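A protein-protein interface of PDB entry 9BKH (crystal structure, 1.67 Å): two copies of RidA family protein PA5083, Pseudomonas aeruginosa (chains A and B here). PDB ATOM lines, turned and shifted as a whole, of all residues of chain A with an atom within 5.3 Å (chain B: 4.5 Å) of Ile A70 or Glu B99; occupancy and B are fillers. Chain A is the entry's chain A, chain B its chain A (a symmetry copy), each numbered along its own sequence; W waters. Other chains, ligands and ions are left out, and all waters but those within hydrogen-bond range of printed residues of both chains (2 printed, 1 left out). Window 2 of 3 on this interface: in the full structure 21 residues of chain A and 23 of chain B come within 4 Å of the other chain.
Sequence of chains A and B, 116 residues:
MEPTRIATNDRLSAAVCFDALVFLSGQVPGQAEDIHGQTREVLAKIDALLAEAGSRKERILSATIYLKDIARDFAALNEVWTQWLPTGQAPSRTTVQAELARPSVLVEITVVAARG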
ATOM      1  N   LEU A  67      -5.954 -23.959  17.103  1.00  0.00           N
ATOM      2  CA  LEU A  67      -5.846 -25.354  16.694  1.00  0.00           C
ATOM      3  C   LEU A  67      -7.215 -25.887  16.321  1.00  0.00           C
ATOM      4  O   LEU A  67      -8.176 -25.713  17.075  1.00  0.00           O
ATOM      5  CB  LEU A  67      -5.240 -26.208  17.822  1.00  0.00           C
ATOM      6  CG  LEU A  67      -3.789 -25.883  18.150  1.00  0.00           C
ATOM      7  CD1 LEU A  67      -3.353 -26.521  19.440  1.00  0.00           C
ATOM      8  CD2 LEU A  67      -2.893 -26.348  17.020  1.00  0.00           C
ATOM      9  N   LYS A  68      -7.306 -26.571  15.184  1.00  0.00           N
ATOM     10  CA  LYS A  68      -8.567 -27.228  14.833  1.00  0.00           C
ATOM     11  C   LYS A  68      -9.005 -28.208  15.921  1.00  0.00           C
ATOM     12  O   LYS A  68     -10.194 -28.307  16.240  1.00  0.00           O
ATOM     13  CB  LYS A  68      -8.428 -27.953  13.486  1.00  0.00           C
ATOM     14  CG  LYS A  68      -9.716 -28.617  12.970  1.00  0.00           C
ATOM     15  CD  LYS A  68      -9.494 -29.259  11.592  1.00  0.00           C
ATOM     16  CE  LYS A  68     -10.623 -30.094  10.999  1.00  0.00           C
ATOM     17  NZ  LYS A  68     -11.865 -30.188  11.788  1.00  0.00           N
ATOM     18  N   ASP A  69      -8.062 -28.969  16.465  1.00  0.00           N
ATOM     19  CA  ASP A  69      -8.316 -29.978  17.489  1.00  0.00           C
ATOM     20  C   ASP A  69      -7.284 -29.815  18.597  1.00  0.00           C
ATOM     21  O   ASP A  69      -6.171 -30.368  18.543  1.00  0.00           O
ATOM     22  CB  ASP A  69      -8.266 -31.363  16.894  1.00  0.00           C
ATOM     23  CG  ASP A  69      -8.771 -32.426  17.860  1.00  0.00           C
ATOM     24  OD1 ASP A  69      -8.633 -32.239  19.081  1.00  0.00           O
ATOM     25  OD2 ASP A  69      -9.303 -33.450  17.387  1.00  0.00           O
ATOM     26  N   ILE A  70      -7.648 -29.055  19.618  1.00  0.00           N
ATOM     27  CA  ILE A  70      -6.671 -28.709  20.628  1.00  0.00           C
ATOM     28  C   ILE A  70      -6.300 -29.937  21.454  1.00  0.00           C
ATOM     29  O   ILE A  70      -5.136 -30.114  21.834  1.00  0.00           O
ATOM     30  CB  ILE A  70      -7.174 -27.535  21.486  1.00  0.00           C
ATOM     31  CG1 ILE A  70      -6.037 -27.022  22.360  1.00  0.00           C
ATOM     32  CG2 ILE A  70      -8.359 -27.923  22.377  1.00  0.00           C
ATOM     33  CD1 ILE A  70      -6.215 -25.619  22.832  1.00  0.00           C
ATOM     34  N   ALA A  71      -7.262 -30.821  21.735  1.00  0.00           N
ATOM     35  CA  ALA A  71      -6.917 -32.009  22.516  1.00  0.00           C
ATOM     36  C   ALA A  71      -5.886 -32.859  21.793  1.00  0.00           C
ATOM     37  O   ALA A  71      -4.952 -33.387  22.410  1.00  0.00           O
ATOM     38  CB  ALA A  71      -8.171 -32.839  22.803  1.00  0.00           C
ATOM     39  N   ARG A  72      -6.027 -32.988  20.483  1.00  0.00           N
ATOM     40  CA  ARG A  72      -5.225 -33.902  19.698  1.00  0.00           C
ATOM     41  C   ARG A  72      -3.847 -33.348  19.389  1.00  0.00           C
ATOM     42  O   ARG A  72      -2.878 -34.108  19.328  1.00  0.00           O
ATOM     43  CB  ARG A  72      -5.943 -34.194  18.396  1.00  0.00           C
ATOM     44  CG  ARG A  72      -5.312 -35.250  17.515  1.00  0.00           C
ATOM     45  CD  ARG A  72      -6.294 -35.605  16.465  1.00  0.00           C
ATOM     46  NE  ARG A  72      -5.852 -36.661  15.572  1.00  0.00           N
ATOM     47  CZ  ARG A  72      -6.641 -37.185  14.648  1.00  0.00           C
ATOM     48  NH1 ARG A  72      -7.891 -36.766  14.501  1.00  0.00           N
ATOM     49  NH2 ARG A  72      -6.167 -38.131  13.838  1.00  0.00           N
ATOM     50  N   ASP A  73      -3.751 -32.043  19.194  1.00  0.00           N
ATOM     51  CA  ASP A  73      -2.568 -31.450  18.586  1.00  0.00           C
ATOM     52  C   ASP A  73      -1.795 -30.494  19.477  1.00  0.00           C
ATOM     53  O   ASP A  73      -0.735 -30.006  19.048  1.00  0.00           O
ATOM     54  CB  ASP A  73      -2.988 -30.723  17.299  1.00  0.00           C
ATOM     55  CG  ASP A  73      -3.343 -31.658  16.192  1.00  0.00           C
ATOM     56  OD1 ASP A  73      -2.837 -32.810  16.156  1.00  0.00           O
ATOM     57  OD2 ASP A  73      -4.135 -31.245  15.336  1.00  0.00           O
ATOM     58  N   PHE A  74      -2.261 -30.236  20.706  1.00  0.00           N
ATOM     59  CA  PHE A  74      -1.577 -29.315  21.604  1.00  0.00           C
ATOM     60  C   PHE A  74      -0.130 -29.745  21.858  1.00  0.00           C
ATOM     61  O   PHE A  74       0.769 -28.900  21.918  1.00  0.00           O
ATOM     62  CB  PHE A  74      -2.361 -29.212  22.924  1.00  0.00           C
ATOM     63  CG  PHE A  74      -1.913 -28.106  23.847  1.00  0.00           C
ATOM     64  CD1 PHE A  74      -1.850 -26.776  23.439  1.00  0.00           C
ATOM     65  CD2 PHE A  74      -1.622 -28.391  25.173  1.00  0.00           C
ATOM     66  CE1 PHE A  74      -1.462 -25.787  24.333  1.00  0.00           C
ATOM     67  CE2 PHE A  74      -1.242 -27.401  26.050  1.00  0.00           C
ATOM     68  CZ  PHE A  74      -1.171 -26.102  25.632  1.00  0.00           C
ATOM     69  N   THR A  95      -3.645 -20.130  23.492  1.00  0.00           N
ATOM     70  CA  THR A  95      -3.858 -21.253  22.591  1.00  0.00           C
ATOM     71  C   THR A  95      -5.283 -21.754  22.787  1.00  0.00           C
ATOM     72  O   THR A  95      -5.658 -22.144  23.901  1.00  0.00           O
ATOM     73  CB  THR A  95      -2.855 -22.386  22.842  1.00  0.00           C
ATOM     74  OG1 THR A  95      -1.520 -21.845  22.852  1.00  0.00           O
ATOM     75  CG2 THR A  95      -2.961 -23.422  21.771  1.00  0.00           C
ATOM     76  N   VAL A  96      -6.077 -21.742  21.713  1.00  0.00           N
ATOM     77  CA  VAL A  96      -7.480 -22.133  21.796  1.00  0.00           C
ATOM     78  C   VAL A  96      -7.850 -22.958  20.576  1.00  0.00           C
ATOM     79  O   VAL A  96      -7.141 -22.992  19.567  1.00  0.00           O
ATOM     80  CB  VAL A  96      -8.429 -20.916  21.929  1.00  0.00           C
ATOM     81  CG1 VAL A  96      -8.021 -20.043  23.085  1.00  0.00           C
ATOM     82  CG2 VAL A  96      -8.466 -20.116  20.602  1.00  0.00           C
ATOM     83  N   GLN A  97      -9.007 -23.625  20.664  1.00  0.00           N
ATOM     84  CA  GLN A  97      -9.517 -24.399  19.558  1.00  0.00           C
ATOM     85  C   GLN A  97     -10.428 -23.536  18.683  1.00  0.00           C
ATOM     86  O   GLN A  97     -11.315 -22.841  19.180  1.00  0.00           O
ATOM     87  CB  GLN A  97     -10.315 -25.604  20.053  1.00  0.00           C
ATOM     88  CG  GLN A  97     -10.900 -26.452  18.948  1.00  0.00           C
ATOM     89  CD  GLN A  97     -11.369 -27.771  19.422  1.00  0.00           C
ATOM     90  OE1 GLN A  97     -10.565 -28.616  19.806  1.00  0.00           O
ATOM     91  NE2 GLN A  97     -12.684 -27.977  19.423  1.00  0.00           N
ATOM     92  N   LYS B  68     -15.666 -22.289  27.064  1.00  0.00           N
ATOM     93  CA  LYS B  68     -15.887 -23.613  26.477  1.00  0.00           C
ATOM     94  C   LYS B  68     -17.318 -23.758  25.958  1.00  0.00           C
ATOM     95  O   LYS B  68     -17.548 -24.346  24.897  1.00  0.00           O
ATOM     96  CB  LYS B  68     -15.581 -24.707  27.509  1.00  0.00           C
ATOM     97  CG  LYS B  68     -15.702 -26.148  26.984  1.00  0.00           C
ATOM     98  CD  LYS B  68     -15.315 -27.167  28.068  1.00  0.00           C
ATOM     99  CE  LYS B  68     -15.523 -28.646  27.770  1.00  0.00           C
ATOM    100  NZ  LYS B  68     -16.049 -28.987  26.434  1.00  0.00           N
ATOM    101  N   ALA B  98     -14.689 -21.195  22.602  1.00  0.00           N
ATOM    102  CA  ALA B  98     -13.566 -21.986  22.126  1.00  0.00           C
ATOM    103  C   ALA B  98     -13.236 -23.018  23.192  1.00  0.00           C
ATOM    104  O   ALA B  98     -13.237 -22.692  24.378  1.00  0.00           O
ATOM    105  CB  ALA B  98     -12.335 -21.130  21.856  1.00  0.00           C
ATOM    106  N   GLU B  99     -12.968 -24.249  22.759  1.00  0.00           N
ATOM    107  CA  GLU B  99     -12.414 -25.251  23.657  1.00  0.00           C
ATOM    108  C   GLU B  99     -11.010 -24.824  24.073  1.00  0.00           C
ATOM    109  O   GLU B  99     -10.229 -24.305  23.255  1.00  0.00           O
ATOM    110  CB  GLU B  99     -12.371 -26.612  22.965  1.00  0.00           C
ATOM    111  CG  GLU B  99     -12.017 -27.703  23.907  1.00  0.00           C
ATOM    112  CD  GLU B  99     -13.235 -28.482  24.330  1.00  0.00           C
ATOM    113  OE1 GLU B  99     -14.387 -28.024  24.065  1.00  0.00           O
ATOM    114  OE2 GLU B  99     -13.029 -29.554  24.935  1.00  0.00           O
ATOM    115  N   LEU B 100     -10.693 -25.007  25.355  1.00  0.00           N
ATOM    116  CA  LEU B 100      -9.379 -24.664  25.887  1.00  0.00           C
ATOM    117  C   LEU B 100      -8.520 -25.926  25.996  1.00  0.00           C
ATOM    118  O   LEU B 100      -8.938 -27.031  25.666  1.00  0.00           O
ATOM    119  CB  LEU B 100      -9.516 -23.953  27.228  1.00  0.00           C
ATOM    120  CG  LEU B 100     -10.236 -22.602  27.303  1.00  0.00           C
ATOM    121  CD1 LEU B 100      -9.876 -21.724  26.115  1.00  0.00           C
ATOM    122  CD2 LEU B 100     -11.740 -22.639  27.442  1.00  0.00           C
ATOM    123  N   ALA B 101      -7.284 -25.750  26.484  1.00  0.00           N
ATOM    124  CA  ALA B 101      -6.299 -26.817  26.342  1.00  0.00           C
ATOM    125  C   ALA B 101      -6.644 -28.051  27.157  1.00  0.00           C
ATOM    126  O   ALA B 101      -6.246 -29.166  26.792  1.00  0.00           O
ATOM    127  CB  ALA B 101      -4.907 -26.315  26.739  1.00  0.00           C
ATOM    128  N   PRO B 103     -10.047 -30.115  28.992  1.00  0.00           N
ATOM    129  CA  PRO B 103     -11.520 -30.108  28.927  1.00  0.00           C
ATOM    130  C   PRO B 103     -12.187 -29.583  30.185  1.00  0.00           C
ATOM    131  O   PRO B 103     -13.332 -29.123  30.110  1.00  0.00           O
ATOM    132  CB  PRO B 103     -11.878 -31.584  28.682  1.00  0.00           C
ATOM    133  CG  PRO B 103     -10.634 -32.243  28.272  1.00  0.00           C
ATOM    134  CD  PRO B 103      -9.484 -31.463  28.809  1.00  0.00           C
HETATM  135  O   HOH W   1      -4.890 -30.403  24.968  1.00  0.00           O
HETATM  136  O   HOH W   2      -5.942 -23.097  26.402  1.00  0.00           O
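The backbone NH (N) of Gln A97 is in hydrogen-bond range of the backbone carbonyl oxygen (O) of Glu B99 (2.9 Å).
The backbone carbonyl oxygen (O) of Val A96 sits at hydrogen-bond distance from the backbone NH (N) of Leu A67 (2.9 Å). The backbone NH (N) of Ile A70 is in hydrogen-bond range of the side-chain amide oxygen (OE1) of Gln A97, 3.0 Å away. OE1 of Glu B99 is in salt-bridge range of NZ of Lys B68 (3.0 Å).
Among the printed residues, pairs that only touch across the chains: Gln A97 with Ala B98 (3.3 Å), Ile A70 with Leu B100 (3.5 Å), Ile A70 with Ala B101 (3.7 Å), Val A96 with Glu B99 (3.8 Å), Phe A74 with Ala B101 (3.9 Å), Val A96 with Ala B98 (3.9 Å), Val A96 with Leu B100 (3.9 Å) and Ile A70 with Glu B99 (3.97 Å).
Asp A69 touches none of the printed residues of chain B. Arg A72 touches none of the printed residues of chain B. Printed residues of chain B within 4 Å of Phe A74: Ala B101. Of the printed residues of chain B, Val A96 touches Ala B98, Glu B99 and Leu B100. Of chain A, only Ile A70 (3.97 Å), Val A96 (3.8 Å) and Gln A97 (2.9 Å) come within 4 Å of Glu B99. Of the printed residues of chain A, Ala B101 touches Ile A70 (3.7 Å) and Phe A74 (3.9 Å). The nearest residue of chain A that does not touch Glu B99 is Thr A95 (5.1 Å). The nearest printed residue of chain A that does not touch Ala B101 is Thr A95 (4.7 Å).
Of the 6 printed residues of chain B, 4 touch a printed residue of chain A. Printed residues of chain B that touch a printed residue of chain A: Ala B98, Glu B99, Leu B100 and Ala B101. Hydrophobic or aromatic side chains of chain B that line the printed part of chain A: Ala B98, Leu B100 and Ala B101. Hydrophobic or aromatic side chains of chain A within 4 Å of the printed part of chain B: Ile A70, Phe A74 and Val A96. Among the printed residues, no Asp or Glu carboxylate lies within 4 Å of a Lys or Arg side-chain nitrogen of the other chain.
Position printed for both chains: 68. Of the 9 pairs that touch across the chains among the printed residues, none has its exchanged pair printed and touching as well.
Water W1 lies within hydrogen-bond range of the backbone carbonyl oxygen of Ala B101 (2.6 Å) and the backbone carbonyl oxygen of Ile A70 (3.2 Å). Water W2 lies within hydrogen-bond range of the backbone carbonyl oxygen of Thr A95 (2.7 Å) and the backbone NH of Ala B101 (3.0 Å).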
